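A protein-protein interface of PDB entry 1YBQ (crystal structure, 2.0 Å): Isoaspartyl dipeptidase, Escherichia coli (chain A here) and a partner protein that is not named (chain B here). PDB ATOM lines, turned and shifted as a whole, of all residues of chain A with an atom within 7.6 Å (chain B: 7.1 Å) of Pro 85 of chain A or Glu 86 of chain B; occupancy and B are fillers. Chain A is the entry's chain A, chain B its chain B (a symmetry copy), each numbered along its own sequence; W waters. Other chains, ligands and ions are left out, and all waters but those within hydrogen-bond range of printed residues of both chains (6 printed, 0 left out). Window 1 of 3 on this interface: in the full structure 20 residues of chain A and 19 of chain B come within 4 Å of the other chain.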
ATOM      1  N   HIS A  70       5.139  26.096  11.598  1.00  0.00           N
ATOM      2  CA  HIS A  70       5.183  24.651  11.484  1.00  0.00           C
ATOM      3  C   HIS A  70       5.580  24.271  10.060  1.00  0.00           C
ATOM      4  O   HIS A  70       4.761  23.783   9.304  1.00  0.00           O
ATOM      5  CB  HIS A  70       3.807  24.043  11.846  1.00  0.00           C
ATOM      6  CG  HIS A  70       3.538  24.357  13.273  1.00  0.00           C
ATOM      7  ND1 HIS A  70       3.815  23.453  14.266  1.00  0.00           N
ATOM      8  CD2 HIS A  70       3.142  25.533  13.855  1.00  0.00           C
ATOM      9  CE1 HIS A  70       3.559  24.069  15.430  1.00  0.00           C
ATOM     10  NE2 HIS A  70       3.136  25.307  15.218  1.00  0.00           N
ATOM     11  N   LEU A  71       6.823  24.544   9.680  1.00  0.00           N
ATOM     12  CA  LEU A  71       7.310  24.257   8.325  1.00  0.00           C
ATOM     13  C   LEU A  71       6.895  22.901   7.705  1.00  0.00           C
ATOM     14  O   LEU A  71       6.679  22.850   6.487  1.00  0.00           O
ATOM     15  CB  LEU A  71       8.840  24.428   8.198  1.00  0.00           C
ATOM     16  CG  LEU A  71       9.343  25.732   8.776  1.00  0.00           C
ATOM     17  CD1 LEU A  71      10.886  25.782   8.726  1.00  0.00           C
ATOM     18  CD2 LEU A  71       8.740  26.757   7.849  1.00  0.00           C
ATOM     19  N   ILE A  72       6.840  21.799   8.506  1.00  0.00           N
ATOM     20  CA  ILE A  72       6.532  20.463   7.977  1.00  0.00           C
ATOM     21  C   ILE A  72       5.102  20.045   8.168  1.00  0.00           C
ATOM     22  O   ILE A  72       4.718  18.947   7.778  1.00  0.00           O
ATOM     23  CB  ILE A  72       7.448  19.328   8.498  1.00  0.00           C
ATOM     24  CG1 ILE A  72       7.306  19.082  10.012  1.00  0.00           C
ATOM     25  CG2 ILE A  72       8.895  19.573   8.092  1.00  0.00           C
ATOM     26  CD1 ILE A  72       8.212  17.996  10.566  1.00  0.00           C
ATOM     27  N   GLY A  73       4.330  20.914   8.789  1.00  0.00           N
ATOM     28  CA  GLY A  73       2.960  20.547   9.057  1.00  0.00           C
ATOM     29  C   GLY A  73       2.864  20.408  10.551  1.00  0.00           C
ATOM     30  O   GLY A  73       3.894  20.323  11.203  1.00  0.00           O
ATOM     31  N   GLY A  74       1.647  20.445  11.074  1.00  0.00           N
ATOM     32  CA  GLY A  74       1.453  20.356  12.494  1.00  0.00           C
ATOM     33  C   GLY A  74       0.148  19.669  12.682  1.00  0.00           C
ATOM     34  O   GLY A  74      -0.188  18.735  11.934  1.00  0.00           O
ATOM     35  N   GLY A  75      -0.585  20.163  13.654  1.00  0.00           N
ATOM     36  CA  GLY A  75      -1.906  19.601  13.919  1.00  0.00           C
ATOM     37  C   GLY A  75      -1.874  18.163  14.466  1.00  0.00           C
ATOM     38  O   GLY A  75      -0.895  17.742  15.052  1.00  0.00           O
ATOM     39  N   PRO A  80      -5.300  11.639  12.833  1.00  0.00           N
ATOM     40  CA  PRO A  80      -4.389  11.747  11.698  1.00  0.00           C
ATOM     41  C   PRO A  80      -4.870  12.554  10.526  1.00  0.00           C
ATOM     42  O   PRO A  80      -4.075  13.114   9.738  1.00  0.00           O
ATOM     43  CB  PRO A  80      -4.073  10.337  11.226  1.00  0.00           C
ATOM     44  CG  PRO A  80      -4.747   9.400  12.206  1.00  0.00           C
ATOM     45  CD  PRO A  80      -5.545  10.237  13.208  1.00  0.00           C
ATOM     46  N   THR A  81      -6.178  12.590  10.380  1.00  0.00           N
ATOM     47  CA  THR A  81      -6.706  13.365   9.275  1.00  0.00           C
ATOM     48  C   THR A  81      -6.451  14.834   9.578  1.00  0.00           C
ATOM     49  O   THR A  81      -6.528  15.664   8.696  1.00  0.00           O
ATOM     50  CB  THR A  81      -8.218  13.103   9.040  1.00  0.00           C
ATOM     51  OG1 THR A  81      -8.964  13.651  10.126  1.00  0.00           O
ATOM     52  CG2 THR A  81      -8.510  11.603   8.883  1.00  0.00           C
ATOM     53  N   THR A  82      -6.156  15.195  10.831  1.00  0.00           N
ATOM     54  CA  THR A  82      -5.923  16.621  11.063  1.00  0.00           C
ATOM     55  C   THR A  82      -4.466  17.043  11.113  1.00  0.00           C
ATOM     56  O   THR A  82      -4.143  18.062  11.712  1.00  0.00           O
ATOM     57  CB  THR A  82      -6.657  17.162  12.283  1.00  0.00           C
ATOM     58  OG1 THR A  82      -6.154  16.507  13.417  1.00  0.00           O
ATOM     59  CG2 THR A  82      -8.115  16.785  12.110  1.00  0.00           C
ATOM     60  N   ARG A  83      -3.604  16.247  10.489  1.00  0.00           N
ATOM     61  CA  ARG A  83      -2.208  16.558  10.356  1.00  0.00           C
ATOM     62  C   ARG A  83      -2.079  17.577   9.217  1.00  0.00           C
ATOM     63  O   ARG A  83      -2.333  17.261   8.046  1.00  0.00           O
ATOM     64  CB  ARG A  83      -1.398  15.306  10.044  1.00  0.00           C
ATOM     65  CG  ARG A  83      -1.349  14.354  11.235  1.00  0.00           C
ATOM     66  CD  ARG A  83      -0.820  12.976  10.843  1.00  0.00           C
ATOM     67  NE  ARG A  83       0.625  13.006  10.745  1.00  0.00           N
ATOM     68  CZ  ARG A  83       1.337  12.921   9.617  1.00  0.00           C
ATOM     69  NH1 ARG A  83       0.777  12.770   8.429  1.00  0.00           N
ATOM     70  NH2 ARG A  83       2.672  12.996   9.677  1.00  0.00           N
ATOM     71  N   THR A  84      -1.697  18.819   9.548  1.00  0.00           N
ATOM     72  CA  THR A  84      -1.619  19.812   8.518  1.00  0.00           C
ATOM     73  C   THR A  84      -0.480  19.544   7.576  1.00  0.00           C
ATOM     74  O   THR A  84       0.440  18.784   7.788  1.00  0.00           O
ATOM     75  CB  THR A  84      -1.627  21.247   9.073  1.00  0.00           C
ATOM     76  OG1 THR A  84      -0.421  21.400   9.732  1.00  0.00           O
ATOM     77  CG2 THR A  84      -2.712  21.394  10.143  1.00  0.00           C
ATOM     78  N   PRO A  85      -0.535  20.211   6.495  1.00  0.00           N
ATOM     79  CA  PRO A  85       0.471  20.071   5.459  1.00  0.00           C
ATOM     80  C   PRO A  85       1.700  20.988   5.618  1.00  0.00           C
ATOM     81  O   PRO A  85       1.749  21.967   6.395  1.00  0.00           O
ATOM     82  CB  PRO A  85      -0.256  20.451   4.187  1.00  0.00           C
ATOM     83  CG  PRO A  85      -1.587  21.099   4.606  1.00  0.00           C
ATOM     84  CD  PRO A  85      -1.764  20.910   6.099  1.00  0.00           C
ATOM     85  N   GLU A  86       2.726  20.639   4.852  1.00  0.00           N
ATOM     86  CA  GLU A  86       3.953  21.378   4.872  1.00  0.00           C
ATOM     87  C   GLU A  86       3.768  22.763   4.297  1.00  0.00           C
ATOM     88  O   GLU A  86       2.794  23.039   3.594  1.00  0.00           O
ATOM     89  CB  GLU A  86       5.117  20.609   4.244  1.00  0.00           C
ATOM     90  CG  GLU A  86       5.091  20.595   2.700  1.00  0.00           C
ATOM     91  CD  GLU A  86       6.260  19.824   2.135  1.00  0.00           C
ATOM     92  OE1 GLU A  86       7.433  20.049   2.434  1.00  0.00           O
ATOM     93  OE2 GLU A  86       5.888  18.880   1.301  1.00  0.00           O
ATOM     94  N   VAL A  87       4.702  23.645   4.631  1.00  0.00           N
ATOM     95  CA  VAL A  87       4.609  25.009   4.193  1.00  0.00           C
ATOM     96  C   VAL A  87       5.271  25.096   2.851  1.00  0.00           C
ATOM     97  O   VAL A  87       6.321  24.490   2.658  1.00  0.00           O
ATOM     98  CB  VAL A  87       5.313  25.964   5.179  1.00  0.00           C
ATOM     99  CG1 VAL A  87       5.395  27.288   4.485  1.00  0.00           C
ATOM    100  CG2 VAL A  87       4.500  26.170   6.469  1.00  0.00           C
ATOM    101  N   ALA A  88       4.654  25.819   1.923  1.00  0.00           N
ATOM    102  CA  ALA A  88       5.240  26.027   0.591  1.00  0.00           C
ATOM    103  C   ALA A  88       5.872  27.410   0.478  1.00  0.00           C
ATOM    104  O   ALA A  88       5.357  28.438   0.944  1.00  0.00           O
ATOM    105  CB  ALA A  88       4.292  25.782  -0.577  1.00  0.00           C
ATOM    106  N   ARG A  91       3.961  30.613  -0.284  1.00  0.00           N
ATOM    107  CA  ARG A  91       3.046  31.085   0.750  1.00  0.00           C
ATOM    108  C   ARG A  91       3.725  32.062   1.669  1.00  0.00           C
ATOM    109  O   ARG A  91       3.096  32.962   2.222  1.00  0.00           O
ATOM    110  CB  ARG A  91       2.581  29.953   1.665  1.00  0.00           C
ATOM    111  CG  ARG A  91       1.512  29.080   1.050  1.00  0.00           C
ATOM    112  CD  ARG A  91       0.120  29.717   1.043  1.00  0.00           C
ATOM    113  NE  ARG A  91      -0.883  28.659   0.965  1.00  0.00           N
ATOM    114  CZ  ARG A  91      -1.048  27.762   1.932  1.00  0.00           C
ATOM    115  NH1 ARG A  91      -0.341  27.829   3.096  1.00  0.00           N
ATOM    116  NH2 ARG A  91      -1.993  26.777   1.771  1.00  0.00           N
ATOM    117  N   ARG A 111       5.712  13.320  13.824  1.00  0.00           N
ATOM    118  CA  ARG A 111       6.531  14.510  13.418  1.00  0.00           C
ATOM    119  C   ARG A 111       7.917  14.397  14.053  1.00  0.00           C
ATOM    120  O   ARG A 111       8.004  14.088  15.239  1.00  0.00           O
ATOM    121  CB  ARG A 111       5.942  15.877  13.785  1.00  0.00           C
ATOM    122  CG  ARG A 111       4.536  16.130  13.272  1.00  0.00           C
ATOM    123  CD  ARG A 111       4.370  16.009  11.757  1.00  0.00           C
ATOM    124  NE  ARG A 111       3.074  16.538  11.322  1.00  0.00           N
ATOM    125  CZ  ARG A 111       2.746  16.741  10.049  1.00  0.00           C
ATOM    126  NH1 ARG A 111       3.567  16.481   9.027  1.00  0.00           N
ATOM    127  NH2 ARG A 111       1.547  17.235   9.791  1.00  0.00           N
ATOM    128  N   GLY A 286       1.939  29.938  11.525  1.00  0.00           N
ATOM    129  CA  GLY A 286       1.534  29.412  10.238  1.00  0.00           C
ATOM    130  C   GLY A 286       1.625  27.892  10.130  1.00  0.00           C
ATOM    131  O   GLY A 286       2.571  27.294  10.594  1.00  0.00           O
ATOM    132  N   ASN A 287       0.615  27.292   9.501  1.00  0.00           N
ATOM    133  CA  ASN A 287       0.494  25.857   9.258  1.00  0.00           C
ATOM    134  C   ASN A 287       0.184  25.057  10.495  1.00  0.00           C
ATOM    135  O   ASN A 287       0.006  23.845  10.441  1.00  0.00           O
ATOM    136  CB  ASN A 287       1.626  25.232   8.444  1.00  0.00           C
ATOM    137  CG  ASN A 287       1.313  25.291   6.980  1.00  0.00           C
ATOM    138  OD1 ASN A 287       0.726  26.269   6.519  1.00  0.00           O
ATOM    139  ND2 ASN A 287       1.786  24.282   6.252  1.00  0.00           N
ATOM    140  N   GLY A 288       0.105  25.743  11.616  1.00  0.00           N
ATOM    141  CA  GLY A 288      -0.223  25.009  12.805  1.00  0.00           C
ATOM    142  C   GLY A 288      -1.726  24.855  12.862  1.00  0.00           C
ATOM    143  O   GLY A 288      -2.466  25.602  12.236  1.00  0.00           O
ATOM    144  N   VAL A 304      -6.635  25.628  10.412  1.00  0.00           N
ATOM    145  CA  VAL A 304      -5.226  25.769  10.140  1.00  0.00           C
ATOM    146  C   VAL A 304      -4.862  27.231   9.870  1.00  0.00           C
ATOM    147  O   VAL A 304      -5.536  27.913   9.109  1.00  0.00           O
ATOM    148  CB  VAL A 304      -4.751  24.824   9.041  1.00  0.00           C
ATOM    149  CG1 VAL A 304      -5.649  24.989   7.847  1.00  0.00           C
ATOM    150  CG2 VAL A 304      -3.346  25.180   8.619  1.00  0.00           C
ATOM    151  N   HIS B  70       4.170   6.400  -2.539  1.00  0.00           N
ATOM    152  CA  HIS B  70       4.900   7.086  -1.477  1.00  0.00           C
ATOM    153  C   HIS B  70       3.986   8.052  -0.795  1.00  0.00           C
ATOM    154  O   HIS B  70       4.054   9.241  -0.992  1.00  0.00           O
ATOM    155  CB  HIS B  70       6.115   7.825  -2.028  1.00  0.00           C
ATOM    156  CG  HIS B  70       7.127   6.839  -2.498  1.00  0.00           C
ATOM    157  ND1 HIS B  70       8.175   6.441  -1.687  1.00  0.00           N
ATOM    158  CD2 HIS B  70       7.232   6.148  -3.685  1.00  0.00           C
ATOM    159  CE1 HIS B  70       8.897   5.556  -2.388  1.00  0.00           C
ATOM    160  NE2 HIS B  70       8.368   5.361  -3.594  1.00  0.00           N
ATOM    161  N   LEU B  71       3.096   7.495  -0.028  1.00  0.00           N
ATOM    162  CA  LEU B  71       2.100   8.308   0.643  1.00  0.00           C
ATOM    163  C   LEU B  71       2.539   9.599   1.348  1.00  0.00           C
ATOM    164  O   LEU B  71       1.789  10.574   1.295  1.00  0.00           O
ATOM    165  CB  LEU B  71       1.237   7.453   1.596  1.00  0.00           C
ATOM    166  CG  LEU B  71       0.444   6.316   0.935  1.00  0.00           C
ATOM    167  CD1 LEU B  71      -0.291   5.558   2.041  1.00  0.00           C
ATOM    168  CD2 LEU B  71      -0.594   6.846  -0.073  1.00  0.00           C
ATOM    169  N   ILE B  72       3.693   9.592   2.044  1.00  0.00           N
ATOM    170  CA  ILE B  72       4.081  10.767   2.799  1.00  0.00           C
ATOM    171  C   ILE B  72       5.044  11.631   2.047  1.00  0.00           C
ATOM    172  O   ILE B  72       5.479  12.663   2.545  1.00  0.00           O
ATOM    173  CB  ILE B  72       4.660  10.460   4.181  1.00  0.00           C
ATOM    174  CG1 ILE B  72       5.804   9.456   4.145  1.00  0.00           C
ATOM    175  CG2 ILE B  72       3.566  10.023   5.140  1.00  0.00           C
ATOM    176  CD1 ILE B  72       6.577   9.434   5.493  1.00  0.00           C
ATOM    177  N   GLY B  73       5.354  11.190   0.845  1.00  0.00           N
ATOM    178  CA  GLY B  73       6.298  11.901   0.035  1.00  0.00           C
ATOM    179  C   GLY B  73       7.519  10.991  -0.055  1.00  0.00           C
ATOM    180  O   GLY B  73       7.612  10.032   0.688  1.00  0.00           O
ATOM    181  N   GLY B  74       8.416  11.293  -0.984  1.00  0.00           N
ATOM    182  CA  GLY B  74       9.622  10.531  -1.251  1.00  0.00           C
ATOM    183  C   GLY B  74      10.686  11.486  -1.737  1.00  0.00           C
ATOM    184  O   GLY B  74      10.820  12.613  -1.225  1.00  0.00           O
ATOM    185  N   ARG B  83      12.557  16.665  -1.942  1.00  0.00           N
ATOM    186  CA  ARG B  83      11.681  15.801  -1.164  1.00  0.00           C
ATOM    187  C   ARG B  83      10.267  16.066  -1.684  1.00  0.00           C
ATOM    188  O   ARG B  83       9.763  17.198  -1.567  1.00  0.00           O
ATOM    189  CB  ARG B  83      11.718  16.161   0.313  1.00  0.00           C
ATOM    190  CG  ARG B  83      13.067  15.708   0.846  1.00  0.00           C
ATOM    191  CD  ARG B  83      13.316  16.362   2.176  1.00  0.00           C
ATOM    192  NE  ARG B  83      12.601  15.672   3.239  1.00  0.00           N
ATOM    193  CZ  ARG B  83      11.546  16.153   3.912  1.00  0.00           C
ATOM    194  NH1 ARG B  83      11.015  17.353   3.654  1.00  0.00           N
ATOM    195  NH2 ARG B  83      11.005  15.419   4.877  1.00  0.00           N
ATOM    196  N   THR B  84       9.625  15.047  -2.262  1.00  0.00           N
ATOM    197  CA  THR B  84       8.303  15.190  -2.825  1.00  0.00           C
ATOM    198  C   THR B  84       7.195  15.314  -1.776  1.00  0.00           C
ATOM    199  O   THR B  84       7.318  14.939  -0.636  1.00  0.00           O
ATOM    200  CB  THR B  84       8.049  14.117  -3.870  1.00  0.00           C
ATOM    201  OG1 THR B  84       7.921  12.960  -3.157  1.00  0.00           O
ATOM    202  CG2 THR B  84       9.294  13.879  -4.719  1.00  0.00           C
ATOM    203  N   PRO B  85       6.082  15.891  -2.161  1.00  0.00           N
ATOM    204  CA  PRO B  85       4.967  16.112  -1.242  1.00  0.00           C
ATOM    205  C   PRO B  85       4.098  14.875  -0.979  1.00  0.00           C
ATOM    206  O   PRO B  85       4.180  13.829  -1.682  1.00  0.00           O
ATOM    207  CB  PRO B  85       4.160  17.232  -1.884  1.00  0.00           C
ATOM    208  CG  PRO B  85       4.770  17.480  -3.259  1.00  0.00           C
ATOM    209  CD  PRO B  85       5.779  16.383  -3.523  1.00  0.00           C
ATOM    210  N   GLU B  86       3.289  14.970   0.086  1.00  0.00           N
ATOM    211  CA  GLU B  86       2.429  13.837   0.450  1.00  0.00           C
ATOM    212  C   GLU B  86       1.333  13.685  -0.574  1.00  0.00           C
ATOM    213  O   GLU B  86       1.029  14.623  -1.304  1.00  0.00           O
ATOM    214  CB  GLU B  86       1.763  14.002   1.828  1.00  0.00           C
ATOM    215  CG  GLU B  86       0.863  15.245   1.924  1.00  0.00           C
ATOM    216  CD  GLU B  86       0.272  15.399   3.311  1.00  0.00           C
ATOM    217  OE1 GLU B  86      -0.264  14.489   3.864  1.00  0.00           O
ATOM    218  OE2 GLU B  86       0.365  16.583   3.862  1.00  0.00           O
ATOM    219  N   VAL B  87       0.730  12.515  -0.616  1.00  0.00           N
ATOM    220  CA  VAL B  87      -0.356  12.265  -1.555  1.00  0.00           C
ATOM    221  C   VAL B  87      -1.696  12.849  -1.055  1.00  0.00           C
ATOM    222  O   VAL B  87      -2.026  12.813   0.140  1.00  0.00           O
ATOM    223  CB  VAL B  87      -0.476  10.773  -1.937  1.00  0.00           C
ATOM    224  CG1 VAL B  87      -1.502  10.592  -3.034  1.00  0.00           C
ATOM    225  CG2 VAL B  87       0.844  10.276  -2.504  1.00  0.00           C
ATOM    226  N   ALA B  88      -2.463  13.447  -1.971  1.00  0.00           N
ATOM    227  CA  ALA B  88      -3.780  14.001  -1.669  1.00  0.00           C
ATOM    228  C   ALA B  88      -4.823  12.959  -2.076  1.00  0.00           C
ATOM    229  O   ALA B  88      -4.657  12.259  -3.068  1.00  0.00           O
ATOM    230  CB  ALA B  88      -4.031  15.269  -2.472  1.00  0.00           C
ATOM    231  N   ARG B  91      -6.337  12.890  -5.618  1.00  0.00           N
ATOM    232  CA  ARG B  91      -5.475  12.448  -6.709  1.00  0.00           C
ATOM    233  C   ARG B  91      -5.541  10.937  -6.918  1.00  0.00           C
ATOM    234  O   ARG B  91      -5.348  10.418  -8.018  1.00  0.00           O
ATOM    235  CB  ARG B  91      -4.044  12.857  -6.418  1.00  0.00           C
ATOM    236  CG  ARG B  91      -3.773  14.307  -6.805  1.00  0.00           C
ATOM    237  CD  ARG B  91      -2.293  14.483  -7.160  1.00  0.00           C
ATOM    238  NE  ARG B  91      -1.492  15.174  -6.118  1.00  0.00           N
ATOM    239  CZ  ARG B  91      -0.781  14.633  -5.118  1.00  0.00           C
ATOM    240  NH1 ARG B  91      -0.686  13.295  -4.893  1.00  0.00           N
ATOM    241  NH2 ARG B  91      -0.105  15.443  -4.275  1.00  0.00           N
ATOM    242  N   ARG B 111      12.445  10.659   6.572  1.00  0.00           N
ATOM    243  CA  ARG B 111      11.172   9.916   6.376  1.00  0.00           C
ATOM    244  C   ARG B 111      11.103   8.821   7.427  1.00  0.00           C
ATOM    245  O   ARG B 111      12.094   8.113   7.617  1.00  0.00           O
ATOM    246  CB  ARG B 111      11.011   9.294   4.985  1.00  0.00           C
ATOM    247  CG  ARG B 111      11.129  10.296   3.827  1.00  0.00           C
ATOM    248  CD  ARG B 111      10.232  11.553   3.962  1.00  0.00           C
ATOM    249  NE  ARG B 111      10.143  12.271   2.665  1.00  0.00           N
ATOM    250  CZ  ARG B 111       9.260  13.208   2.317  1.00  0.00           C
ATOM    251  NH1 ARG B 111       8.325  13.656   3.164  1.00  0.00           N
ATOM    252  NH2 ARG B 111       9.335  13.718   1.080  1.00  0.00           N
ATOM    253  N   LYS B 119      -0.399   8.667   8.225  1.00  0.00           N
ATOM    254  CA  LYS B 119      -0.972   8.973   6.905  1.00  0.00           C
ATOM    255  C   LYS B 119      -1.935   7.872   6.389  1.00  0.00           C
ATOM    256  O   LYS B 119      -3.035   8.134   5.890  1.00  0.00           O
ATOM    257  CB  LYS B 119       0.161   9.271   5.909  1.00  0.00           C
ATOM    258  CG  LYS B 119      -0.325   9.644   4.506  1.00  0.00           C
ATOM    259  CD  LYS B 119      -1.268  10.855   4.467  1.00  0.00           C
ATOM    260  CE  LYS B 119      -1.516  11.376   3.046  1.00  0.00           C
ATOM    261  NZ  LYS B 119      -2.214  12.679   2.924  1.00  0.00           N
ATOM    262  N   ALA B 122      -4.870   8.190   8.194  1.00  0.00           N
ATOM    263  CA  ALA B 122      -5.637   9.351   7.767  1.00  0.00           C
ATOM    264  C   ALA B 122      -6.471   8.952   6.557  1.00  0.00           C
ATOM    265  O   ALA B 122      -7.646   9.252   6.463  1.00  0.00           O
ATOM    266  CB  ALA B 122      -4.720  10.549   7.445  1.00  0.00           C
ATOM    267  N   ASN B 287       3.985   9.665  -6.428  1.00  0.00           N
ATOM    268  CA  ASN B 287       4.617  10.574  -5.471  1.00  0.00           C
ATOM    269  C   ASN B 287       6.059  10.314  -5.229  1.00  0.00           C
ATOM    270  O   ASN B 287       6.701  11.017  -4.472  1.00  0.00           O
ATOM    271  CB  ASN B 287       3.867  10.883  -4.162  1.00  0.00           C
ATOM    272  CG  ASN B 287       2.959  12.053  -4.393  1.00  0.00           C
ATOM    273  OD1 ASN B 287       2.043  11.940  -5.219  1.00  0.00           O
ATOM    274  ND2 ASN B 287       3.262  13.169  -3.742  1.00  0.00           N
ATOM    275  N   PHE B 387      -7.237  18.588   4.216  1.00  0.00           N
ATOM    276  CA  PHE B 387      -6.461  19.796   3.878  1.00  0.00           C
ATOM    277  C   PHE B 387      -6.098  19.927   2.425  1.00  0.00           C
ATOM    278  O   PHE B 387      -4.981  20.335   2.090  1.00  0.00           O
ATOM    279  CB  PHE B 387      -5.177  19.940   4.687  1.00  0.00           C
ATOM    280  CG  PHE B 387      -5.563  20.094   6.108  1.00  0.00           C
ATOM    281  CD1 PHE B 387      -5.189  19.143   7.052  1.00  0.00           C
ATOM    282  CD2 PHE B 387      -6.347  21.176   6.511  1.00  0.00           C
ATOM    283  CE1 PHE B 387      -5.604  19.314   8.377  1.00  0.00           C
ATOM    284  CE2 PHE B 387      -6.764  21.358   7.831  1.00  0.00           C
ATOM    285  CZ  PHE B 387      -6.383  20.406   8.777  1.00  0.00           C
ATOM    286  N   GLU B 388      -7.055  19.584   1.587  1.00  0.00           N
ATOM    287  CA  GLU B 388      -6.895  19.687   0.157  1.00  0.00           C
ATOM    288  C   GLU B 388      -7.455  21.024  -0.356  1.00  0.00           C
ATOM    289  O   GLU B 388      -8.523  21.477   0.122  1.00  0.00           O
ATOM    290  CB  GLU B 388      -7.648  18.528  -0.510  1.00  0.00           C
ATOM    291  CG  GLU B 388      -6.867  17.217  -0.576  1.00  0.00           C
ATOM    292  CD  GLU B 388      -7.359  16.436  -1.746  1.00  0.00           C
ATOM    293  OE1 GLU B 388      -7.953  15.384  -1.622  1.00  0.00           O
ATOM    294  OE2 GLU B 388      -7.132  17.059  -2.891  1.00  0.00           O
HETATM  295  O   HOH W   1       3.597  17.218   1.557  1.00  0.00           O
HETATM  296  O   HOH W   2      -1.696  17.335   5.080  1.00  0.00           O
HETATM  297  O   HOH W   3       8.495  18.416   4.515  1.00  0.00           O
HETATM  298  O   HOH W   4       7.338  16.267   1.862  1.00  0.00           O
HETATM  299  O   HOH W   5       1.807  16.897   6.513  1.00  0.00           O
HETATM  300  O   HOH W   6       1.977  18.375   3.098  1.00  0.00           O
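The backbone carbonyl oxygen of Thr 84 of chain A lies within hydrogen-bond range of the guanidinium group of Arg 111 of chain A, at 2.8 Å. The backbone NH of Gly 74 of chain A lies within hydrogen-bond range of the side-chain hydroxyl of Thr 84 of chain A, at 2.6 Å. O of Glu 86 of chain B is in hydrogen-bond range of NH2 of Arg 91 of chain B, 3.3 Å away. OE1 of Glu 86 of chain B is in salt-bridge range of NZ of Lys 119 of chain B, 2.8 Å away. The backbone carbonyl oxygen (O) of Asn 287 of chain A sits at hydrogen-bond distance from the side-chain hydroxyl (OG1) of Thr 84 of chain A (2.6 Å). The backbone carbonyl oxygen (O) of Glu 86 of chain A is in hydrogen-bond range of the side-chain amide nitrogen (ND2) of Asn 287 of chain A (3.1 Å).
Among the printed residues, pairs that only touch across the chains: Thr 81 of chain A with Ala 122 of chain B (3.5 Å), Pro 80 of chain A with Ala 122 of chain B (3.5 Å), Arg 83 of chain A with Phe 387 of chain B (3.6 Å), Thr 82 of chain A with Phe 387 of chain B (3.7 Å), Pro 85 of chain A with Phe 387 of chain B (3.8 Å), Thr 81 of chain A with Phe 387 of chain B (3.8 Å), Val 304 of chain A with Phe 387 of chain B (3.8 Å), Pro 85 of chain A with Glu 86 of chain B (3.8 Å), Glu 86 of chain A with Pro 85 of chain B (3.9 Å) and Thr 84 of chain A with Phe 387 of chain B (3.9 Å).
Printed residues of chain B within 4 Å of Pro 80 of chain A: Ala 122. Of the printed residues of chain B, Arg 83 of chain A touches Phe 387. Of the printed residues of chain B, Val 304 of chain A touches Phe 387. Thr 84 of chain B touches none of the printed residues of chain A. Glu 86 of chain B touches just one residue of chain A: Pro 85. The nearest residue of chain B that does not touch Pro 85 of chain A is Glu 388 of chain B (6.4 Å).
Among the printed residues, 10 pairs touch across the chains. Among the printed residues, no Asp or Glu carboxylate lies within 4 Å of a Lys or Arg side-chain nitrogen of the other chain.
Water W2 lies within hydrogen-bond range of the side-chain carboxylate of Glu 86 of chain B and the backbone carbonyl oxygen of Arg 83 of chain A. Water W6 bridges the side-chain carboxylate of Glu 86 of chain B (2.5 Å) and the backbone NH of Glu 86 of chain A (3.0 Å). Water W5 lies within hydrogen-bond range of the backbone carbonyl oxygen of Thr 84 of chain A (2.7 Å), the side-chain carboxylate of Glu 86 of chain B (3.0 Å) and the guanidinium group of Arg 111 of chain A (3.1 Å). Water W1 bridges the backbone NH of Glu 86 of chain B and the side-chain carboxylate of Glu 86 of chain A. Water W4 lies within hydrogen-bond range of the backbone carbonyl oxygen (O) of Thr 84 of chain B (2.8 Å), the side-chain carboxylate (OE2) of Glu 86 of chain A (3.0 Å) and the guanidinium group (NH1) of Arg 111 of chain B (3.1 Å). Water W3 bridges the side-chain carboxylate (OE1) of Glu 86 of chain A (2.9 Å) and the guanidinium group (NH1) of Arg 83 of chain B (2.9 Å).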
